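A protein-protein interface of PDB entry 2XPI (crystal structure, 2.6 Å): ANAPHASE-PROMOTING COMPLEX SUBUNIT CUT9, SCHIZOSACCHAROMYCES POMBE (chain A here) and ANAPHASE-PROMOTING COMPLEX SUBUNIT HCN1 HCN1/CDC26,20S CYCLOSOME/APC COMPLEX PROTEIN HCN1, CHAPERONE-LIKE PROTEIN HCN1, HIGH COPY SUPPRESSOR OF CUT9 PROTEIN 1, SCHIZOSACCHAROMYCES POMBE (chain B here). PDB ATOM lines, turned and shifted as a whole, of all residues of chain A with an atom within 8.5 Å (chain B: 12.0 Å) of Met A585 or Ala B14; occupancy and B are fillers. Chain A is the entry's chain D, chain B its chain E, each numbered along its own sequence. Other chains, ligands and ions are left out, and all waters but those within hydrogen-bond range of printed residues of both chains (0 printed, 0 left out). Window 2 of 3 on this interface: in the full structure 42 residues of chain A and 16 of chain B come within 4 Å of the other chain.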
ATOM      1  N   ALA A 550       4.590  -1.633 -12.059  1.00  0.00           N
ATOM      2  CA  ALA A 550       4.223  -0.762 -13.176  1.00  0.00           C
ATOM      3  C   ALA A 550       5.242   0.336 -13.460  1.00  0.00           C
ATOM      4  O   ALA A 550       5.426   0.747 -14.608  1.00  0.00           O
ATOM      5  CB  ALA A 550       2.856  -0.146 -12.938  1.00  0.00           C
ATOM      6  N   ASN A 551       5.897   0.820 -12.411  1.00  0.00           N
ATOM      7  CA  ASN A 551       6.751   1.989 -12.549  1.00  0.00           C
ATOM      8  C   ASN A 551       8.019   1.696 -13.329  1.00  0.00           C
ATOM      9  O   ASN A 551       8.454   2.532 -14.124  1.00  0.00           O
ATOM     10  CB  ASN A 551       7.088   2.617 -11.196  1.00  0.00           C
ATOM     11  CG  ASN A 551       7.828   3.938 -11.343  1.00  0.00           C
ATOM     12  OD1 ASN A 551       9.060   3.991 -11.253  1.00  0.00           O
ATOM     13  ND2 ASN A 551       7.082   5.010 -11.590  1.00  0.00           N
ATOM     14  N   THR A 554       7.170   1.578 -16.974  1.00  0.00           N
ATOM     15  CA  THR A 554       7.156   2.978 -17.399  1.00  0.00           C
ATOM     16  C   THR A 554       8.586   3.501 -17.542  1.00  0.00           C
ATOM     17  O   THR A 554       8.927   4.113 -18.545  1.00  0.00           O
ATOM     18  CB  THR A 554       6.417   3.863 -16.378  1.00  0.00           C
ATOM     19  OG1 THR A 554       5.094   3.359 -16.172  1.00  0.00           O
ATOM     20  CG2 THR A 554       6.339   5.306 -16.868  1.00  0.00           C
ATOM     21  N   ALA A 555       9.409   3.261 -16.521  1.00  0.00           N
ATOM     22  CA  ALA A 555      10.826   3.595 -16.561  1.00  0.00           C
ATOM     23  C   ALA A 555      11.464   3.074 -17.844  1.00  0.00           C
ATOM     24  O   ALA A 555      11.986   3.852 -18.647  1.00  0.00           O
ATOM     25  CB  ALA A 555      11.529   3.003 -15.362  1.00  0.00           C
ATOM     26  N   ALA A 557      10.095   1.850 -20.587  1.00  0.00           N
ATOM     27  CA  ALA A 557       9.472   2.446 -21.767  1.00  0.00           C
ATOM     28  C   ALA A 557      10.127   3.774 -22.133  1.00  0.00           C
ATOM     29  O   ALA A 557      10.527   3.973 -23.281  1.00  0.00           O
ATOM     30  CB  ALA A 557       7.981   2.635 -21.551  1.00  0.00           C
ATOM     31  N   LEU A 558      10.241   4.673 -21.155  1.00  0.00           N
ATOM     32  CA  LEU A 558      10.831   5.984 -21.382  1.00  0.00           C
ATOM     33  C   LEU A 558      12.261   5.874 -21.901  1.00  0.00           C
ATOM     34  O   LEU A 558      12.685   6.679 -22.737  1.00  0.00           O
ATOM     35  CB  LEU A 558      10.803   6.840 -20.112  1.00  0.00           C
ATOM     36  CG  LEU A 558      11.621   8.136 -20.204  1.00  0.00           C
ATOM     37  CD1 LEU A 558      11.081   9.059 -21.294  1.00  0.00           C
ATOM     38  CD2 LEU A 558      11.669   8.865 -18.871  1.00  0.00           C
ATOM     39  N   LEU A 561      11.922   5.159 -25.683  1.00  0.00           N
ATOM     40  CA  LEU A 561      11.655   6.387 -26.408  1.00  0.00           C
ATOM     41  C   LEU A 561      12.960   7.146 -26.642  1.00  0.00           C
ATOM     42  O   LEU A 561      13.252   7.559 -27.758  1.00  0.00           O
ATOM     43  CB  LEU A 561      10.649   7.243 -25.648  1.00  0.00           C
ATOM     44  CG  LEU A 561       9.272   6.595 -25.465  1.00  0.00           C
ATOM     45  CD1 LEU A 561       8.309   7.559 -24.800  1.00  0.00           C
ATOM     46  CD2 LEU A 561       8.725   6.145 -26.800  1.00  0.00           C
ATOM     47  N   LEU A 573       4.781  -0.148 -21.995  1.00  0.00           N
ATOM     48  CA  LEU A 573       3.721   0.716 -21.499  1.00  0.00           C
ATOM     49  C   LEU A 573       2.404  -0.051 -21.432  1.00  0.00           C
ATOM     50  O   LEU A 573       1.553   0.237 -20.590  1.00  0.00           O
ATOM     51  CB  LEU A 573       3.589   1.979 -22.356  1.00  0.00           C
ATOM     52  CG  LEU A 573       4.685   3.030 -22.130  1.00  0.00           C
ATOM     53  CD1 LEU A 573       4.777   4.016 -23.289  1.00  0.00           C
ATOM     54  CD2 LEU A 573       4.489   3.757 -20.810  1.00  0.00           C
ATOM     55  N   SER A 576       2.568  -2.110 -18.106  1.00  0.00           N
ATOM     56  CA  SER A 576       2.373  -1.310 -16.900  1.00  0.00           C
ATOM     57  C   SER A 576       0.971  -0.708 -16.799  1.00  0.00           C
ATOM     58  O   SER A 576       0.465  -0.505 -15.699  1.00  0.00           O
ATOM     59  CB  SER A 576       3.449  -0.228 -16.748  1.00  0.00           C
ATOM     60  OG  SER A 576       3.264   0.826 -17.668  1.00  0.00           O
ATOM     61  N   SER A 580      -1.342  -1.196 -13.574  1.00  0.00           N
ATOM     62  CA  SER A 580      -2.007  -0.064 -12.938  1.00  0.00           C
ATOM     63  C   SER A 580      -2.733   0.759 -14.005  1.00  0.00           C
ATOM     64  O   SER A 580      -2.143   1.638 -14.625  1.00  0.00           O
ATOM     65  CB  SER A 580      -0.982   0.796 -12.201  1.00  0.00           C
ATOM     66  OG  SER A 580      -1.552   2.009 -11.740  1.00  0.00           O
ATOM     67  N   ASN A 582      -4.833   3.128 -14.256  1.00  0.00           N
ATOM     68  CA  ASN A 582      -5.138   4.551 -14.157  1.00  0.00           C
ATOM     69  C   ASN A 582      -3.917   5.451 -14.332  1.00  0.00           C
ATOM     70  O   ASN A 582      -4.052   6.657 -14.547  1.00  0.00           O
ATOM     71  CB  ASN A 582      -5.826   4.852 -12.821  1.00  0.00           C
ATOM     72  CG  ASN A 582      -6.970   3.893 -12.521  1.00  0.00           C
ATOM     73  OD1 ASN A 582      -6.748   2.735 -12.158  1.00  0.00           O
ATOM     74  ND2 ASN A 582      -8.201   4.374 -12.667  1.00  0.00           N
ATOM     75  N   GLU A 583      -2.730   4.853 -14.246  1.00  0.00           N
ATOM     76  CA  GLU A 583      -1.469   5.592 -14.280  1.00  0.00           C
ATOM     77  C   GLU A 583      -1.483   6.777 -15.250  1.00  0.00           C
ATOM     78  O   GLU A 583      -1.642   6.612 -16.464  1.00  0.00           O
ATOM     79  CB  GLU A 583      -0.300   4.652 -14.588  1.00  0.00           C
ATOM     80  N   ILE A 584      -1.315   7.972 -14.691  1.00  0.00           N
ATOM     81  CA  ILE A 584      -1.350   9.211 -15.460  1.00  0.00           C
ATOM     82  C   ILE A 584      -0.112   9.375 -16.350  1.00  0.00           C
ATOM     83  O   ILE A 584      -0.220   9.812 -17.498  1.00  0.00           O
ATOM     84  CB  ILE A 584      -1.487  10.447 -14.535  1.00  0.00           C
ATOM     85  N   MET A 585       1.058   9.027 -15.819  1.00  0.00           N
ATOM     86  CA  MET A 585       2.311   9.141 -16.567  1.00  0.00           C
ATOM     87  C   MET A 585       2.432   8.057 -17.630  1.00  0.00           C
ATOM     88  O   MET A 585       2.925   8.305 -18.730  1.00  0.00           O
ATOM     89  CB  MET A 585       3.517   9.079 -15.629  1.00  0.00           C
ATOM     90  CG  MET A 585       3.673  10.288 -14.733  1.00  0.00           C
ATOM     91  SD  MET A 585       4.921   9.987 -13.476  1.00  0.00           S
ATOM     92  CE  MET A 585       4.395   8.379 -12.867  1.00  0.00           C
ATOM     93  N   ALA A 586       1.994   6.852 -17.291  1.00  0.00           N
ATOM     94  CA  ALA A 586       1.985   5.769 -18.257  1.00  0.00           C
ATOM     95  C   ALA A 586       1.181   6.212 -19.467  1.00  0.00           C
ATOM     96  O   ALA A 586       1.667   6.178 -20.598  1.00  0.00           O
ATOM     97  CB  ALA A 586       1.380   4.522 -17.647  1.00  0.00           C
ATOM     98  N   SER A 587      -0.046   6.655 -19.215  1.00  0.00           N
ATOM     99  CA  SER A 587      -0.970   7.011 -20.282  1.00  0.00           C
ATOM    100  C   SER A 587      -0.424   8.098 -21.204  1.00  0.00           C
ATOM    101  O   SER A 587      -0.438   7.939 -22.423  1.00  0.00           O
ATOM    102  CB  SER A 587      -2.318   7.430 -19.701  1.00  0.00           C
ATOM    103  OG  SER A 587      -3.322   7.360 -20.693  1.00  0.00           O
ATOM    104  N   ASP A 588       0.050   9.201 -20.627  1.00  0.00           N
ATOM    105  CA  ASP A 588       0.627  10.292 -21.420  1.00  0.00           C
ATOM    106  C   ASP A 588       1.840   9.807 -22.196  1.00  0.00           C
ATOM    107  O   ASP A 588       1.941  10.004 -23.410  1.00  0.00           O
ATOM    108  CB  ASP A 588       1.023  11.476 -20.536  1.00  0.00           C
ATOM    109  CG  ASP A 588      -0.170  12.310 -20.107  1.00  0.00           C
ATOM    110  OD1 ASP A 588      -1.315  11.824 -20.228  1.00  0.00           O
ATOM    111  OD2 ASP A 588       0.035  13.453 -19.646  1.00  0.00           O
ATOM    112  N   LEU A 589       2.754   9.162 -21.483  1.00  0.00           N
ATOM    113  CA  LEU A 589       3.967   8.623 -22.081  1.00  0.00           C
ATOM    114  C   LEU A 589       3.641   7.665 -23.236  1.00  0.00           C
ATOM    115  O   LEU A 589       4.403   7.553 -24.197  1.00  0.00           O
ATOM    116  CB  LEU A 589       4.806   7.929 -21.003  1.00  0.00           C
ATOM    117  CG  LEU A 589       6.320   7.884 -21.206  1.00  0.00           C
ATOM    118  CD1 LEU A 589       6.843   9.247 -21.610  1.00  0.00           C
ATOM    119  CD2 LEU A 589       7.006   7.401 -19.943  1.00  0.00           C
ATOM    120  N   LEU A 590       2.497   6.991 -23.145  1.00  0.00           N
ATOM    121  CA  LEU A 590       2.082   6.059 -24.189  1.00  0.00           C
ATOM    122  C   LEU A 590       1.699   6.775 -25.479  1.00  0.00           C
ATOM    123  O   LEU A 590       2.294   6.525 -26.528  1.00  0.00           O
ATOM    124  CB  LEU A 590       0.925   5.176 -23.717  1.00  0.00           C
ATOM    125  CG  LEU A 590       0.202   4.372 -24.803  1.00  0.00           C
ATOM    126  CD1 LEU A 590       1.174   3.761 -25.795  1.00  0.00           C
ATOM    127  CD2 LEU A 590      -0.642   3.294 -24.176  1.00  0.00           C
ATOM    128  N   LYS A 591       0.702   7.654 -25.399  1.00  0.00           N
ATOM    129  CA  LYS A 591       0.232   8.383 -26.573  1.00  0.00           C
ATOM    130  C   LYS A 591       1.403   8.867 -27.427  1.00  0.00           C
ATOM    131  O   LYS A 591       1.349   8.809 -28.658  1.00  0.00           O
ATOM    132  CB  LYS A 591      -0.653   9.561 -26.165  1.00  0.00           C
ATOM    133  N   ARG A 592       2.468   9.319 -26.768  1.00  0.00           N
ATOM    134  CA  ARG A 592       3.636   9.858 -27.462  1.00  0.00           C
ATOM    135  C   ARG A 592       4.428   8.788 -28.235  1.00  0.00           C
ATOM    136  O   ARG A 592       4.920   9.037 -29.339  1.00  0.00           O
ATOM    137  CB  ARG A 592       4.536  10.600 -26.472  1.00  0.00           C
ATOM    138  N   ALA B   9      12.744   3.825  -3.315  1.00  0.00           N
ATOM    139  CA  ALA B   9      12.787   3.641  -4.742  1.00  0.00           C
ATOM    140  C   ALA B   9      12.538   4.960  -5.451  1.00  0.00           C
ATOM    141  O   ALA B   9      11.492   5.564  -5.295  1.00  0.00           O
ATOM    142  CB  ALA B   9      11.750   2.621  -5.154  1.00  0.00           C
ATOM    143  N   ILE B  10      13.503   5.411  -6.239  1.00  0.00           N
ATOM    144  CA  ILE B  10      13.227   6.505  -7.147  1.00  0.00           C
ATOM    145  C   ILE B  10      12.092   6.054  -8.080  1.00  0.00           C
ATOM    146  O   ILE B  10      12.073   4.898  -8.523  1.00  0.00           O
ATOM    147  CB  ILE B  10      14.469   6.856  -7.958  1.00  0.00           C
ATOM    148  CG1 ILE B  10      15.613   7.245  -7.028  1.00  0.00           C
ATOM    149  CG2 ILE B  10      14.171   7.974  -8.941  1.00  0.00           C
ATOM    150  CD1 ILE B  10      16.982   6.992  -7.641  1.00  0.00           C
ATOM    151  N   GLN B  11      11.145   6.952  -8.355  1.00  0.00           N
ATOM    152  CA  GLN B  11      10.013   6.660  -9.234  1.00  0.00           C
ATOM    153  C   GLN B  11      10.042   7.550 -10.463  1.00  0.00           C
ATOM    154  O   GLN B  11      10.772   8.533 -10.498  1.00  0.00           O
ATOM    155  CB  GLN B  11       8.704   6.896  -8.495  1.00  0.00           C
ATOM    156  CG  GLN B  11       8.485   5.961  -7.330  1.00  0.00           C
ATOM    157  CD  GLN B  11       8.063   4.579  -7.782  1.00  0.00           C
ATOM    158  OE1 GLN B  11       8.889   3.673  -7.926  1.00  0.00           O
ATOM    159  NE2 GLN B  11       6.768   4.413  -8.021  1.00  0.00           N
ATOM    160  N   ILE B  12       9.236   7.217 -11.468  1.00  0.00           N
ATOM    161  CA  ILE B  12       9.134   8.059 -12.659  1.00  0.00           C
ATOM    162  C   ILE B  12       8.242   9.274 -12.417  1.00  0.00           C
ATOM    163  O   ILE B  12       7.162   9.152 -11.842  1.00  0.00           O
ATOM    164  CB  ILE B  12       8.628   7.279 -13.873  1.00  0.00           C
ATOM    165  CG1 ILE B  12       9.743   6.389 -14.421  1.00  0.00           C
ATOM    166  CG2 ILE B  12       8.188   8.234 -14.958  1.00  0.00           C
ATOM    167  CD1 ILE B  12      10.938   7.150 -14.922  1.00  0.00           C
ATOM    168  N   THR B  13       8.706  10.441 -12.865  1.00  0.00           N
ATOM    169  CA  THR B  13       8.031  11.718 -12.599  1.00  0.00           C
ATOM    170  C   THR B  13       7.526  12.417 -13.873  1.00  0.00           C
ATOM    171  O   THR B  13       8.044  12.196 -14.972  1.00  0.00           O
ATOM    172  CB  THR B  13       8.969  12.715 -11.870  1.00  0.00           C
ATOM    173  OG1 THR B  13       9.737  13.441 -12.837  1.00  0.00           O
ATOM    174  CG2 THR B  13       9.910  11.995 -10.922  1.00  0.00           C
ATOM    175  N   ALA B  14       6.516  13.272 -13.707  1.00  0.00           N
ATOM    176  CA  ALA B  14       6.051  14.123 -14.795  1.00  0.00           C
ATOM    177  C   ALA B  14       7.208  14.970 -15.320  1.00  0.00           C
ATOM    178  O   ALA B  14       7.304  15.230 -16.520  1.00  0.00           O
ATOM    179  CB  ALA B  14       4.914  15.003 -14.328  1.00  0.00           C
ATOM    180  N   GLU B  15       8.091  15.393 -14.422  1.00  0.00           N
ATOM    181  CA  GLU B  15       9.278  16.127 -14.833  1.00  0.00           C
ATOM    182  C   GLU B  15      10.082  15.255 -15.786  1.00  0.00           C
ATOM    183  O   GLU B  15      10.806  15.750 -16.654  1.00  0.00           O
ATOM    184  CB  GLU B  15      10.125  16.516 -13.616  1.00  0.00           C
ATOM    185  CG  GLU B  15      11.551  16.949 -13.944  1.00  0.00           C
ATOM    186  N   ASP B  16       9.938  13.944 -15.621  1.00  0.00           N
ATOM    187  CA  ASP B  16      10.659  12.984 -16.447  1.00  0.00           C
ATOM    188  C   ASP B  16      10.089  12.922 -17.871  1.00  0.00           C
ATOM    189  O   ASP B  16      10.843  12.799 -18.846  1.00  0.00           O
ATOM    190  CB  ASP B  16      10.663  11.599 -15.783  1.00  0.00           C
ATOM    191  CG  ASP B  16      11.671  11.495 -14.641  1.00  0.00           C
ATOM    192  OD1 ASP B  16      12.779  12.066 -14.766  1.00  0.00           O
ATOM    193  OD2 ASP B  16      11.358  10.838 -13.621  1.00  0.00           O
ATOM    194  N   VAL B  17       8.762  13.015 -17.985  1.00  0.00           N
ATOM    195  CA  VAL B  17       8.120  13.073 -19.292  1.00  0.00           C
ATOM    196  C   VAL B  17       8.455  14.407 -19.952  1.00  0.00           C
ATOM    197  O   VAL B  17       8.817  14.448 -21.134  1.00  0.00           O
ATOM    198  CB  VAL B  17       6.586  12.868 -19.212  1.00  0.00           C
ATOM    199  CG1 VAL B  17       6.220  12.002 -18.009  1.00  0.00           C
ATOM    200  CG2 VAL B  17       5.862  14.194 -19.146  1.00  0.00           C
ATOM    201  N   LEU B  18       8.354  15.487 -19.169  1.00  0.00           N
ATOM    202  CA  LEU B  18       8.730  16.834 -19.605  1.00  0.00           C
ATOM    203  C   LEU B  18      10.176  16.841 -20.057  1.00  0.00           C
ATOM    204  O   LEU B  18      10.516  17.404 -21.095  1.00  0.00           O
ATOM    205  CB  LEU B  18       8.561  17.840 -18.464  1.00  0.00           C
ATOM    206  CG  LEU B  18       7.179  18.425 -18.139  1.00  0.00           C
ATOM    207  CD1 LEU B  18       6.042  17.424 -18.361  1.00  0.00           C
ATOM    208  CD2 LEU B  18       7.151  18.975 -16.709  1.00  0.00           C
ATOM    209  N   ALA B  19      11.030  16.212 -19.261  1.00  0.00           N
ATOM    210  CA  ALA B  19      12.434  16.070 -19.611  1.00  0.00           C
ATOM    211  C   ALA B  19      12.593  15.477 -21.013  1.00  0.00           C
ATOM    212  O   ALA B  19      13.382  15.975 -21.820  1.00  0.00           O
ATOM    213  CB  ALA B  19      13.144  15.205 -18.578  1.00  0.00           C
ATOM    214  N   TYR B  20      11.845  14.410 -21.289  1.00  0.00           N
ATOM    215  CA  TYR B  20      11.864  13.769 -22.603  1.00  0.00           C
ATOM    216  C   TYR B  20      11.425  14.747 -23.683  1.00  0.00           C
ATOM    217  O   TYR B  20      12.090  14.901 -24.713  1.00  0.00           O
ATOM    218  CB  TYR B  20      10.951  12.536 -22.637  1.00  0.00           C
ATOM    219  CG  TYR B  20      10.859  11.929 -24.014  1.00  0.00           C
ATOM    220  CD1 TYR B  20      12.011  11.564 -24.700  1.00  0.00           C
ATOM    221  CD2 TYR B  20       9.634  11.733 -24.638  1.00  0.00           C
ATOM    222  CE1 TYR B  20      11.954  11.018 -25.970  1.00  0.00           C
ATOM    223  CE2 TYR B  20       9.560  11.182 -25.916  1.00  0.00           C
ATOM    224  CZ  TYR B  20      10.729  10.825 -26.579  1.00  0.00           C
ATOM    225  OH  TYR B  20      10.694  10.273 -27.847  1.00  0.00           O
ATOM    226  N   ASP B  21      10.295  15.403 -23.430  1.00  0.00           N
ATOM    227  CA  ASP B  21       9.712  16.369 -24.357  1.00  0.00           C
ATOM    228  C   ASP B  21      10.701  17.448 -24.795  1.00  0.00           C
ATOM    229  O   ASP B  21      10.405  18.237 -25.686  1.00  0.00           O
ATOM    230  CB  ASP B  21       8.447  16.992 -23.758  1.00  0.00           C
ATOM    231  CG  ASP B  21       7.328  15.972 -23.577  1.00  0.00           C
ATOM    232  OD1 ASP B  21       7.515  14.797 -23.968  1.00  0.00           O
ATOM    233  OD2 ASP B  21       6.260  16.346 -23.047  1.00  0.00           O
ATOM    234  N   GLU B  22      11.871  17.480 -24.166  1.00  0.00           N
ATOM    235  CA  GLU B  22      13.006  18.189 -24.740  1.00  0.00           C
ATOM    236  C   GLU B  22      13.584  17.305 -25.852  1.00  0.00           C
ATOM    237  O   GLU B  22      14.784  17.004 -25.880  1.00  0.00           O
ATOM    238  CB  GLU B  22      14.060  18.503 -23.681  1.00  0.00           C
ATOM    239  CG  GLU B  22      15.202  19.361 -24.186  1.00  0.00           C
ATOM    240  N   GLU B  23      12.692  16.872 -26.745  1.00  0.00           N
ATOM    241  CA  GLU B  23      13.042  16.129 -27.952  1.00  0.00           C
ATOM    242  C   GLU B  23      13.422  17.127 -29.053  1.00  0.00           C
ATOM    243  O   GLU B  23      14.058  16.769 -30.048  1.00  0.00           O
ATOM    244  CB  GLU B  23      11.856  15.259 -28.393  1.00  0.00           C
ATOM    245  CG  GLU B  23      12.143  14.318 -29.553  1.00  0.00           C
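The side-chain amide oxygen of Gln B11 sits close to the side-chain amide oxygen of Asn A551 (3.3 Å).
The side-chain sulfur (SD) of Met A585 is in hydrogen-bond range of the backbone NH (N) of Ala B14, 3.7 Å away.
O of Ile B12 lies close to SD of Met A585 (2.9 Å).
The side-chain amide nitrogen of Asn A551 lies close to the backbone NH of Ile B12 (3.1 Å).
The side-chain carboxylate of Asp B16 sits at hydrogen-bond distance from the backbone NH of Thr B13 (2.8 Å).
O of Ala A550 sits at hydrogen-bond distance from OG1 of Thr A554, at 3.1 Å.
The backbone NH (N) of Glu B15 lies within hydrogen-bond range of the side-chain hydroxyl (OG1) of Thr B13, 3.0 Å away.
The side-chain hydroxyl (OG1) of Thr A554 sits at hydrogen-bond distance from the side-chain hydroxyl (OG) of Ser A576, 3.5 Å away.
Among the printed residues, merely in contact across the chains: Met A585 with Thr B13 (3.6 Å), Ala A555 with Ile B12 (3.7 Å), Leu A561 with Tyr B20 (3.7 Å), Leu A558 with Tyr B20 (3.7 Å) and Thr A554 with Ile B12 (3.95 Å).
Asn A551 touches just these residues of chain B: Gln B11 and Ile B12.
Of the printed residues of chain B, Ala A555 touches Ile B12 (3.7 Å).
No residue of chain B comes within 4 Å of Glu A583.
No residue of chain B comes within 4 Å of Ile A584.
Met A585 touches just these residues of chain B: Ile B12, Thr B13 and Ala B14.
No residue of chain B comes within 4 Å of Ala A586.
No residue of chain B comes within 4 Å of Asp A588.
Printed residues of chain A within 4 Å of Ile B12: Asn A551 (3.1 Å), Thr A554 (3.95 Å), Ala A555 (3.7 Å) and Met A585 (2.9 Å).
Glu B23 touches none of the printed residues of chain A.
The nearest residue of chain A that does not touch Ala B14 is Asp A588 (7.4 Å).
Among the printed residues, 9 pairs touch across the chains.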
